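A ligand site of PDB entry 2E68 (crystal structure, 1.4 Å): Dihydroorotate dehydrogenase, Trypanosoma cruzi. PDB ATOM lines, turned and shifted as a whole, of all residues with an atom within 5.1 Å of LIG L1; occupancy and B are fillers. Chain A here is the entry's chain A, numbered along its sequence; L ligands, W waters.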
ATOM      1  N   ALA A  20      13.280 -25.859 -17.568  1.00  0.00           N
ATOM      2  CA  ALA A  20      13.204 -25.722 -16.129  1.00  0.00           C
ATOM      3  C   ALA A  20      11.748 -25.922 -15.705  1.00  0.00           C
ATOM      4  O   ALA A  20      10.840 -25.500 -16.420  1.00  0.00           O
ATOM      5  CB  ALA A  20      13.692 -24.339 -15.703  1.00  0.00           C
ATOM      6  N   ALA A  21      11.524 -26.547 -14.551  1.00  0.00           N
ATOM      7  CA  ALA A  21      10.144 -26.732 -14.096  1.00  0.00           C
ATOM      8  C   ALA A  21       9.418 -25.400 -14.039  1.00  0.00           C
ATOM      9  O   ALA A  21       9.998 -24.363 -13.662  1.00  0.00           O
ATOM     10  CB  ALA A  21      10.112 -27.417 -12.751  1.00  0.00           C
ATOM     11  N   GLY A  22       8.160 -25.423 -14.457  1.00  0.00           N
ATOM     12  CA  GLY A  22       7.329 -24.225 -14.473  1.00  0.00           C
ATOM     13  C   GLY A  22       7.246 -23.517 -15.801  1.00  0.00           C
ATOM     14  O   GLY A  22       6.296 -22.772 -16.042  1.00  0.00           O
ATOM     15  N   VAL A  23       8.242 -23.714 -16.667  1.00  0.00           N
ATOM     16  CA  VAL A  23       8.277 -23.051 -17.966  1.00  0.00           C
ATOM     17  C   VAL A  23       7.847 -24.032 -19.061  1.00  0.00           C
ATOM     18  O   VAL A  23       8.413 -25.114 -19.185  1.00  0.00           O
ATOM     19  CB  VAL A  23       9.675 -22.454 -18.254  1.00  0.00           C
ATOM     20  CG1 VAL A  23       9.714 -21.818 -19.634  1.00  0.00           C
ATOM     21  CG2 VAL A  23      10.034 -21.431 -17.170  1.00  0.00           C
ATOM     22  N   LYS A  45       5.150 -28.932 -14.716  1.00  0.00           N
ATOM     23  CA  LYS A  45       4.945 -27.861 -13.727  1.00  0.00           C
ATOM     24  C   LYS A  45       4.846 -28.410 -12.312  1.00  0.00           C
ATOM     25  O   LYS A  45       4.143 -29.395 -12.093  1.00  0.00           O
ATOM     26  CB  LYS A  45       3.649 -27.102 -14.082  1.00  0.00           C
ATOM     27  CG  LYS A  45       3.118 -26.122 -13.008  1.00  0.00           C
ATOM     28  CD  LYS A  45       4.037 -24.905 -12.873  1.00  0.00           C
ATOM     29  CE  LYS A  45       3.689 -24.066 -11.651  1.00  0.00           C
ATOM     30  NZ  LYS A  45       4.714 -22.979 -11.453  1.00  0.00           N
ATOM     31  N   SER A  46       5.501 -27.780 -11.338  1.00  0.00           N
ATOM     32  CA  SER A  46       5.351 -28.209  -9.949  1.00  0.00           C
ATOM     33  C   SER A  46       3.877 -28.209  -9.573  1.00  0.00           C
ATOM     34  O   SER A  46       3.172 -27.196  -9.754  1.00  0.00           O
ATOM     35  CB  SER A  46       6.131 -27.324  -8.985  1.00  0.00           C
ATOM     36  OG  SER A  46       7.522 -27.541  -9.121  1.00  0.00           O
ATOM     37  N   TYR A  60       4.395 -12.344 -13.853  1.00  0.00           N
ATOM     38  CA  TYR A  60       5.665 -12.652 -14.518  1.00  0.00           C
ATOM     39  C   TYR A  60       6.043 -11.448 -15.377  1.00  0.00           C
ATOM     40  O   TYR A  60       5.196 -10.938 -16.118  1.00  0.00           O
ATOM     41  CB  TYR A  60       5.563 -13.890 -15.400  1.00  0.00           C
ATOM     42  CG  TYR A  60       6.793 -14.106 -16.262  1.00  0.00           C
ATOM     43  CD1 TYR A  60       6.846 -13.612 -17.577  1.00  0.00           C
ATOM     44  CD2 TYR A  60       7.909 -14.777 -15.766  1.00  0.00           C
ATOM     45  CE1 TYR A  60       7.990 -13.787 -18.363  1.00  0.00           C
ATOM     46  CE2 TYR A  60       9.053 -14.965 -16.548  1.00  0.00           C
ATOM     47  CZ  TYR A  60       9.083 -14.472 -17.843  1.00  0.00           C
ATOM     48  OH  TYR A  60      10.225 -14.642 -18.616  1.00  0.00           O
ATOM     49  N   SER A  67      14.293 -12.266 -15.445  1.00  0.00           N
ATOM     50  CA  SER A  67      12.871 -12.247 -15.142  1.00  0.00           C
ATOM     51  C   SER A  67      12.606 -12.192 -13.649  1.00  0.00           C
ATOM     52  O   SER A  67      13.473 -12.535 -12.831  1.00  0.00           O
ATOM     53  CB  SER A  67      12.194 -13.490 -15.740  1.00  0.00           C
ATOM     54  OG  SER A  67      12.614 -14.654 -15.045  1.00  0.00           O
ATOM     55  N   ASN A  69       9.226 -13.372 -11.072  1.00  0.00           N
ATOM     56  CA  ASN A  69       7.955 -14.060 -11.094  1.00  0.00           C
ATOM     57  C   ASN A  69       7.444 -14.345  -9.698  1.00  0.00           C
ATOM     58  O   ASN A  69       8.214 -14.642  -8.792  1.00  0.00           O
ATOM     59  CB  ASN A  69       8.007 -15.368 -11.909  1.00  0.00           C
ATOM     60  CG  ASN A  69       8.373 -16.587 -11.069  1.00  0.00           C
ATOM     61  OD1 ASN A  69       7.521 -17.205 -10.403  1.00  0.00           O
ATOM     62  ND2 ASN A  69       9.653 -16.987 -11.111  1.00  0.00           N
ATOM     63  N   MET A  71       4.429 -16.609  -9.528  1.00  0.00           N
ATOM     64  CA  MET A  71       3.318 -17.356 -10.122  1.00  0.00           C
ATOM     65  C   MET A  71       2.361 -17.886  -9.042  1.00  0.00           C
ATOM     66  O   MET A  71       1.136 -17.786  -9.200  1.00  0.00           O
ATOM     67  CB  MET A  71       3.791 -18.516 -11.001  1.00  0.00           C
ATOM     68  CG  MET A  71       4.785 -18.133 -12.093  1.00  0.00           C
ATOM     69  SD  MET A  71       4.253 -16.844 -13.228  1.00  0.00           S
ATOM     70  CE  MET A  71       3.010 -17.722 -14.157  1.00  0.00           C
ATOM     71  N   LEU A  73       2.417 -21.196  -7.851  1.00  0.00           N
ATOM     72  CA  LEU A  73       2.086 -22.596  -8.182  1.00  0.00           C
ATOM     73  C   LEU A  73       0.719 -22.784  -8.882  1.00  0.00           C
ATOM     74  O   LEU A  73      -0.044 -23.685  -8.505  1.00  0.00           O
ATOM     75  CB  LEU A  73       2.203 -23.509  -6.953  1.00  0.00           C
ATOM     76  CG  LEU A  73       3.597 -23.664  -6.345  1.00  0.00           C
ATOM     77  CD1 LEU A  73       3.522 -24.432  -5.026  1.00  0.00           C
ATOM     78  CD2 LEU A  73       4.577 -24.351  -7.314  1.00  0.00           C
ATOM     79  N   SER A  99       7.470 -32.854 -11.432  1.00  0.00           N
ATOM     80  CA  SER A  99       7.815 -32.033 -10.283  1.00  0.00           C
ATOM     81  C   SER A  99       6.617 -31.891  -9.352  1.00  0.00           C
ATOM     82  O   SER A  99       5.497 -31.622  -9.804  1.00  0.00           O
ATOM     83  CB  SER A  99       8.267 -30.632 -10.725  1.00  0.00           C
ATOM     84  OG  SER A  99       8.542 -29.839  -9.579  1.00  0.00           O
ATOM     85  N   GLU A 127      10.928 -35.095  -9.340  1.00  0.00           N
ATOM     86  CA  GLU A 127      11.693 -33.948  -8.822  1.00  0.00           C
ATOM     87  C   GLU A 127      10.882 -33.305  -7.702  1.00  0.00           C
ATOM     88  O   GLU A 127       9.809 -32.761  -7.951  1.00  0.00           O
ATOM     89  CB  GLU A 127      12.019 -32.917  -9.935  1.00  0.00           C
ATOM     90  CG  GLU A 127      13.013 -31.789  -9.506  1.00  0.00           C
ATOM     91  CD  GLU A 127      13.439 -30.839 -10.656  1.00  0.00           C
ATOM     92  OE1 GLU A 127      12.706 -29.881 -10.960  1.00  0.00           O
ATOM     93  OE2 GLU A 127      14.544 -31.005 -11.218  1.00  0.00           O
ATOM     94  N   ASN A 129      10.222 -30.472  -5.231  1.00  0.00           N
ATOM     95  CA  ASN A 129      10.544 -29.042  -5.147  1.00  0.00           C
ATOM     96  C   ASN A 129      10.545 -28.540  -3.703  1.00  0.00           C
ATOM     97  O   ASN A 129       9.483 -28.418  -3.089  1.00  0.00           O
ATOM     98  CB  ASN A 129       9.534 -28.252  -5.997  1.00  0.00           C
ATOM     99  CG  ASN A 129       9.824 -26.766  -6.035  1.00  0.00           C
ATOM    100  OD1 ASN A 129      10.742 -26.258  -5.389  1.00  0.00           O
ATOM    101  ND2 ASN A 129       9.051 -26.053  -6.832  1.00  0.00           N
ATOM    102  N   LYS A 166      14.766 -30.213  -6.107  1.00  0.00           N
ATOM    103  CA  LYS A 166      14.991 -28.864  -6.633  1.00  0.00           C
ATOM    104  C   LYS A 166      15.359 -27.966  -5.453  1.00  0.00           C
ATOM    105  O   LYS A 166      14.529 -27.718  -4.559  1.00  0.00           O
ATOM    106  CB  LYS A 166      13.736 -28.355  -7.358  1.00  0.00           C
ATOM    107  CG  LYS A 166      13.867 -26.975  -7.995  1.00  0.00           C
ATOM    108  CD  LYS A 166      14.811 -26.961  -9.191  1.00  0.00           C
ATOM    109  CE  LYS A 166      14.730 -25.655 -10.001  1.00  0.00           C
ATOM    110  NZ  LYS A 166      13.452 -25.527 -10.752  1.00  0.00           N
ATOM    111  N   VAL A 195      19.734 -24.225  -9.703  1.00  0.00           N
ATOM    112  CA  VAL A 195      18.958 -23.702  -8.582  1.00  0.00           C
ATOM    113  C   VAL A 195      17.559 -23.286  -9.036  1.00  0.00           C
ATOM    114  O   VAL A 195      17.314 -23.013 -10.224  1.00  0.00           O
ATOM    115  CB  VAL A 195      19.650 -22.450  -7.954  1.00  0.00           C
ATOM    116  CG1 VAL A 195      20.951 -22.846  -7.289  1.00  0.00           C
ATOM    117  CG2 VAL A 195      19.879 -21.354  -8.992  1.00  0.00           C
ATOM    118  N   ASN A 196      16.652 -23.215  -8.073  1.00  0.00           N
ATOM    119  CA  ASN A 196      15.396 -22.489  -8.235  1.00  0.00           C
ATOM    120  C   ASN A 196      15.680 -20.976  -8.306  1.00  0.00           C
ATOM    121  O   ASN A 196      16.840 -20.547  -8.172  1.00  0.00           O
ATOM    122  CB  ASN A 196      14.458 -22.839  -7.061  1.00  0.00           C
ATOM    123  CG  ASN A 196      12.977 -22.784  -7.439  1.00  0.00           C
ATOM    124  OD1 ASN A 196      12.515 -21.831  -8.078  1.00  0.00           O
ATOM    125  ND2 ASN A 196      12.225 -23.806  -7.042  1.00  0.00           N
ATOM    126  N   SER A 197      14.633 -20.176  -8.523  1.00  0.00           N
ATOM    127  CA  SER A 197      14.816 -18.729  -8.643  1.00  0.00           C
ATOM    128  C   SER A 197      15.411 -18.131  -7.366  1.00  0.00           C
ATOM    129  O   SER A 197      15.273 -18.678  -6.261  1.00  0.00           O
ATOM    130  CB  SER A 197      13.490 -18.047  -8.984  1.00  0.00           C
ATOM    131  OG  SER A 197      12.526 -18.286  -7.973  1.00  0.00           O
ATOM    132  N   LEU A 222      13.871 -14.297  -8.889  1.00  0.00           N
ATOM    133  CA  LEU A 222      14.649 -13.831 -10.040  1.00  0.00           C
ATOM    134  C   LEU A 222      15.230 -14.987 -10.833  1.00  0.00           C
ATOM    135  O   LEU A 222      15.736 -15.965 -10.269  1.00  0.00           O
ATOM    136  CB  LEU A 222      15.789 -12.909  -9.591  1.00  0.00           C
ATOM    137  CG  LEU A 222      15.396 -11.716  -8.716  1.00  0.00           C
ATOM    138  CD1 LEU A 222      16.639 -11.031  -8.169  1.00  0.00           C
ATOM    139  CD2 LEU A 222      14.502 -10.720  -9.456  1.00  0.00           C
ATOM    140  N   GLY A 223      15.185 -14.850 -12.151  1.00  0.00           N
ATOM    141  CA  GLY A 223      15.856 -15.775 -13.051  1.00  0.00           C
ATOM    142  C   GLY A 223      16.587 -15.034 -14.159  1.00  0.00           C
ATOM    143  O   GLY A 223      16.485 -13.807 -14.288  1.00  0.00           O
ATOM    144  N   GLY A 224      17.348 -15.780 -14.966  1.00  0.00           N
ATOM    145  CA  GLY A 224      18.032 -15.211 -16.124  1.00  0.00           C
ATOM    146  C   GLY A 224      19.439 -14.736 -15.839  1.00  0.00           C
ATOM    147  O   GLY A 224      20.142 -15.273 -14.964  1.00  0.00           O
ATOM    148  N   ILE A 227      21.342 -14.265 -12.436  1.00  0.00           N
ATOM    149  CA  ILE A 227      21.594 -15.340 -11.483  1.00  0.00           C
ATOM    150  C   ILE A 227      22.664 -16.352 -11.903  1.00  0.00           C
ATOM    151  O   ILE A 227      22.936 -17.288 -11.160  1.00  0.00           O
ATOM    152  CB  ILE A 227      20.273 -16.068 -11.024  1.00  0.00           C
ATOM    153  CG1 ILE A 227      19.764 -17.060 -12.069  1.00  0.00           C
ATOM    154  CG2 ILE A 227      19.206 -15.029 -10.636  1.00  0.00           C
ATOM    155  CD1 ILE A 227      18.829 -18.092 -11.490  1.00  0.00           C
ATOM    156  N   CYS A 250      20.639 -25.327 -13.317  1.00  0.00           N
ATOM    157  CA  CYS A 250      19.546 -24.471 -13.750  1.00  0.00           C
ATOM    158  C   CYS A 250      19.876 -23.066 -13.292  1.00  0.00           C
ATOM    159  O   CYS A 250      20.240 -22.852 -12.132  1.00  0.00           O
ATOM    160  CB  CYS A 250      18.230 -24.925 -13.139  1.00  0.00           C
ATOM    161  SG  CYS A 250      16.777 -24.078 -13.778  1.00  0.00           S
ATOM    162  N   GLY A 251      19.764 -22.107 -14.202  1.00  0.00           N
ATOM    163  CA  GLY A 251      19.926 -20.713 -13.832  1.00  0.00           C
ATOM    164  C   GLY A 251      20.819 -19.979 -14.817  1.00  0.00           C
ATOM    165  O   GLY A 251      22.004 -20.310 -14.976  1.00  0.00           O
ATOM    166  N   GLY A 252      20.232 -19.017 -15.505  1.00  0.00           N
ATOM    167  CA  GLY A 252      21.003 -18.121 -16.347  1.00  0.00           C
ATOM    168  C   GLY A 252      21.490 -18.682 -17.668  1.00  0.00           C
ATOM    169  O   GLY A 252      22.386 -18.095 -18.286  1.00  0.00           O
ATOM    170  N   VAL A 253      20.890 -19.783 -18.148  1.00  0.00           N
ATOM    171  CA  VAL A 253      21.329 -20.359 -19.426  1.00  0.00           C
ATOM    172  C   VAL A 253      20.603 -19.699 -20.605  1.00  0.00           C
ATOM    173  O   VAL A 253      19.372 -19.823 -20.741  1.00  0.00           O
ATOM    174  CB  VAL A 253      21.127 -21.906 -19.473  1.00  0.00           C
ATOM    175  CG1 VAL A 253      21.502 -22.475 -20.848  1.00  0.00           C
ATOM    176  CG2 VAL A 253      21.941 -22.576 -18.388  1.00  0.00           C
ATOM    177  N   GLN A 271      19.077 -27.190 -17.364  1.00  0.00           N
ATOM    178  CA  GLN A 271      17.687 -26.764 -17.517  1.00  0.00           C
ATOM    179  C   GLN A 271      17.644 -25.304 -17.925  1.00  0.00           C
ATOM    180  O   GLN A 271      18.531 -24.511 -17.569  1.00  0.00           O
ATOM    181  CB  GLN A 271      16.906 -26.965 -16.221  1.00  0.00           C
ATOM    182  CG  GLN A 271      17.089 -28.330 -15.584  1.00  0.00           C
ATOM    183  CD  GLN A 271      16.149 -28.563 -14.420  1.00  0.00           C
ATOM    184  OE1 GLN A 271      15.738 -27.622 -13.744  1.00  0.00           O
ATOM    185  NE2 GLN A 271      15.824 -29.813 -14.164  1.00  0.00           N
ATOM    186  N   VAL A 272      16.591 -24.953 -18.665  1.00  0.00           N
ATOM    187  CA  VAL A 272      16.452 -23.627 -19.257  1.00  0.00           C
ATOM    188  C   VAL A 272      15.079 -23.055 -18.881  1.00  0.00           C
ATOM    189  O   VAL A 272      14.045 -23.624 -19.248  1.00  0.00           O
ATOM    190  CB  VAL A 272      16.623 -23.671 -20.793  1.00  0.00           C
ATOM    191  CG1 VAL A 272      16.661 -22.276 -21.369  1.00  0.00           C
ATOM    192  CG2 VAL A 272      17.882 -24.480 -21.171  1.00  0.00           C
ATOM    193  N   GLY A 273      15.080 -21.942 -18.157  1.00  0.00           N
ATOM    194  CA  GLY A 273      13.850 -21.316 -17.675  1.00  0.00           C
ATOM    195  C   GLY A 273      13.537 -20.045 -18.424  1.00  0.00           C
ATOM    196  O   GLY A 273      12.906 -20.057 -19.488  1.00  0.00           O
ATOM    197  N   THR A 274      13.993 -18.918 -17.873  1.00  0.00           N
ATOM    198  CA  THR A 274      13.760 -17.599 -18.449  1.00  0.00           C
ATOM    199  C   THR A 274      14.013 -17.538 -19.953  1.00  0.00           C
ATOM    200  O   THR A 274      13.179 -17.032 -20.706  1.00  0.00           O
ATOM    201  CB  THR A 274      14.581 -16.512 -17.705  1.00  0.00           C
ATOM    202  OG1 THR A 274      14.174 -16.471 -16.331  1.00  0.00           O
ATOM    203  CG2 THR A 274      14.363 -15.125 -18.324  1.00  0.00           C
ATOM    204  N   ALA A 275      15.163 -18.041 -20.408  1.00  0.00           N
ATOM    205  CA  ALA A 275      15.501 -17.923 -21.825  1.00  0.00           C
ATOM    206  C   ALA A 275      14.497 -18.681 -22.690  1.00  0.00           C
ATOM    207  O   ALA A 275      14.183 -18.240 -23.804  1.00  0.00           O
ATOM    208  CB  ALA A 275      16.905 -18.418 -22.100  1.00  0.00           C
HETATM  209  N1  LIG L   1      10.716 -23.960 -10.496  1.00  0.00           N
HETATM  210  C1  LIG L   1      10.153 -25.082  -9.941  1.00  0.00           C
HETATM  211  O1  LIG L   1      10.864 -25.902  -9.355  1.00  0.00           O
HETATM  212  N2  LIG L   1       8.803 -25.299 -10.075  1.00  0.00           N
HETATM  213  C2  LIG L   1       7.961 -24.427 -10.733  1.00  0.00           C
HETATM  214  O2  LIG L   1       6.787 -24.768 -10.982  1.00  0.00           O
HETATM  215  C3  LIG L   1       8.536 -23.295 -11.304  1.00  0.00           C
HETATM  216  N3  LIG L   1       7.768 -22.375 -11.995  1.00  0.00           N
HETATM  217  C4  LIG L   1       8.362 -21.288 -12.609  1.00  0.00           C
HETATM  218  C5  LIG L   1       7.586 -20.364 -13.310  1.00  0.00           C
HETATM  219  C6  LIG L   1       8.178 -19.245 -13.919  1.00  0.00           C
HETATM  220  C7  LIG L   1       7.367 -18.525 -14.967  1.00  0.00           C
HETATM  221  C8  LIG L   1       9.561 -19.054 -13.794  1.00  0.00           C
HETATM  222  C9  LIG L   1      10.285 -18.066 -14.676  1.00  0.00           C
HETATM  223  C10 LIG L   1      10.322 -19.969 -13.068  1.00  0.00           C
HETATM  224  C11 LIG L   1       9.733 -21.079 -12.476  1.00  0.00           C
HETATM  225  N4  LIG L   1      10.502 -21.976 -11.739  1.00  0.00           N
HETATM  226  C12 LIG L   1       9.918 -23.081 -11.178  1.00  0.00           C
HETATM  227  C13 LIG L   1      11.937 -21.698 -11.459  1.00  0.00           C
HETATM  228  C14 LIG L   1      12.735 -22.257 -12.641  1.00  0.00           C
HETATM  229  O3  LIG L   1      12.548 -23.660 -12.748  1.00  0.00           O
HETATM  230  C15 LIG L   1      14.232 -21.968 -12.550  1.00  0.00           C
HETATM  231  O4  LIG L   1      14.711 -22.650 -11.408  1.00  0.00           O
HETATM  232  C16 LIG L   1      14.558 -20.480 -12.446  1.00  0.00           C
HETATM  233  O5  LIG L   1      13.701 -19.729 -13.293  1.00  0.00           O
HETATM  234  C17 LIG L   1      16.022 -20.185 -12.764  1.00  0.00           C
HETATM  235  O6  LIG L   1      16.351 -20.563 -14.084  1.00  0.00           O
HETATM  236  P1  LIG L   1      16.492 -19.467 -15.260  1.00  0.00           P
HETATM  237  O7  LIG L   1      17.577 -18.493 -14.860  1.00  0.00           O
HETATM  238  O8  LIG L   1      16.783 -20.262 -16.514  1.00  0.00           O
HETATM  239  O9  LIG L   1      15.161 -18.743 -15.343  1.00  0.00           O
HETATM  240  O1  LG2 L   2      10.324 -19.306  -9.324  1.00  0.00           O
HETATM  241  C1  LG2 L   2       9.459 -20.140  -9.019  1.00  0.00           C
HETATM  242  N1  LG2 L   2       8.172 -19.894  -9.259  1.00  0.00           N
HETATM  243  N2  LG2 L   2       9.824 -21.284  -8.424  1.00  0.00           N
HETATM  244  C2  LG2 L   2       8.973 -22.202  -7.944  1.00  0.00           C
HETATM  245  O2  LG2 L   2       9.352 -23.252  -7.446  1.00  0.00           O
HETATM  246  C3  LG2 L   2       7.499 -21.935  -8.044  1.00  0.00           C
HETATM  247  C4  LG2 L   2       7.154 -20.944  -9.143  1.00  0.00           C
HETATM  248  C5  LG2 L   2       5.777 -20.431  -8.854  1.00  0.00           C
HETATM  249  O3  LG2 L   2       5.642 -19.328  -8.280  1.00  0.00           O
HETATM  250  O4  LG2 L   2       4.819 -21.163  -9.213  1.00  0.00           O
HETATM  251  O   HOH W   1      18.971 -21.777 -16.894  1.00  0.00           O
HETATM  252  O   HOH W   2       4.473 -21.583 -13.972  1.00  0.00           O
HETATM  253  O   HOH W   3      17.337 -18.923 -18.862  1.00  0.00           O
HETATM  254  O   HOH W   4      10.889 -28.738  -9.342  1.00  0.00           O
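Water W3 lies within hydrogen-bond range of O8 of LIG L1, N of Ala 275, O of Val 253 and N of Thr 274. Water W4 lies within hydrogen-bond range of OG of Ser 99 (2.6 Å), OE1 of Glu 127 (2.7 Å) and O1 of LIG L1 (2.8 Å). Water W2 bridges NZ of Lys 45 (2.9 Å) and O of Gly 22 (3.0 Å).
Ala 20 touches LIG L1. CA of Gly 22 touches N3 of LIG L1, at 3.1 Å. Tyr 60 touches LIG L1. Asn 69 touches LIG L1 (ND2 to C8, 3.4 Å). Met 71 touches LIG L1. Ser 197 touches LIG L1 (N to O4, 3.8 Å). Gly 223 touches LIG L1 (C to O7, 3.7 Å). Ile 227 touches LIG L1. Gly 251 touches LIG L1. Of the 31 residues printed, 21 come within 4 Å of LIG L1.
N of Thr 274 is in hydrogen-bond range of O9 of LIG L1. The side-chain hydroxyl of Thr 274 is in hydrogen-bond range of an oxygen (O9) of LIG L1, at 2.7 Å. The backbone NH of Gly 224 is in hydrogen-bond range of an oxygen (O7) of LIG L1 (2.7 Å). The backbone NH (N) of Ser 46 sits at hydrogen-bond distance from an oxygen (O2) of LIG L1, 3.3 Å away. A nitrogen (N2) of LIG L1 sits at hydrogen-bond distance from the side-chain hydroxyl of Ser 46 (2.8 Å). The side-chain amino group of Lys 45 sits at hydrogen-bond distance from an oxygen (O2) of LIG L1, 2.8 Å away. N of Gly 252 sits at hydrogen-bond distance from O7 of LIG L1 (2.8 Å). The backbone carbonyl oxygen (O) of Ala 21 sits close to an oxygen (O3) of LIG L1 (2.8 Å). An oxygen (O3) of LIG L1 sits at hydrogen-bond distance from the side-chain amino group (NZ) of Lys 166 (2.9 Å). An oxygen (O4) of LIG L1 is in hydrogen-bond range of the backbone carbonyl oxygen (O) of Val 195 (2.9 Å). N of Gly 273 is in hydrogen-bond range of O8 of LIG L1, 2.9 Å away. ND2 of Asn 129 lies within hydrogen-bond range of O1 of LIG L1, 3.1 Å away. O1 of LIG L1 sits at hydrogen-bond distance from ND2 of Asn 196. The side-chain sulfur of Cys 250 lies within hydrogen-bond range of an oxygen (O4) of LIG L1 (3.5 Å). NZ of Lys 45 lies within salt-bridge range of O4 of LG2 L2 (2.9 Å). ND2 of Asn 129 is in hydrogen-bond range of O2 of LG2 L2 (2.9 Å). N2 of LG2 L2 is in hydrogen-bond range of OD1 of Asn 196 (2.8 Å). OD1 of Asn 69 lies within hydrogen-bond range of N1 of LG2 L2. An oxygen (O3) of LG2 L2 lies within hydrogen-bond range of the backbone NH (N) of Met 71 (3.2 Å). OG of Ser 197 is in hydrogen-bond range of O1 of LG2 L2, 2.8 Å away. The backbone NH (N) of Leu 73 lies within hydrogen-bond range of an oxygen (O4) of LG2 L2 (2.8 Å).
N2 of LIG L1 lies close to O2 of LG2 L2 (3.4 Å).
The side-chain hydroxyl of Thr 274 is in hydrogen-bond range of the side-chain hydroxyl of Ser 67, at 2.7 Å. The side-chain hydroxyl (OG) of Ser 46 sits at hydrogen-bond distance from the side-chain amide nitrogen (ND2) of Asn 129, at 3.1 Å. The backbone NH (N) of Val 195 lies within hydrogen-bond range of the backbone carbonyl oxygen (O) of Cys 250, at 2.8 Å. The side-chain amide oxygen (OD1) of Asn 129 lies within hydrogen-bond range of the side-chain amide nitrogen (ND2) of Asn 196 (3.3 Å). The backbone NH (N) of Ala 20 sits at hydrogen-bond distance from the backbone carbonyl oxygen (O) of Val 272 (2.9 Å). OD1 of Asn 69 sits at hydrogen-bond distance from N of Met 71 (3.3 Å). The side-chain sulfur (SG) of Cys 250 is in hydrogen-bond range of the side-chain amide oxygen (OE1) of Gln 271 (3.7 Å). O of Gly 223 sits at hydrogen-bond distance from N of Ser 67.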
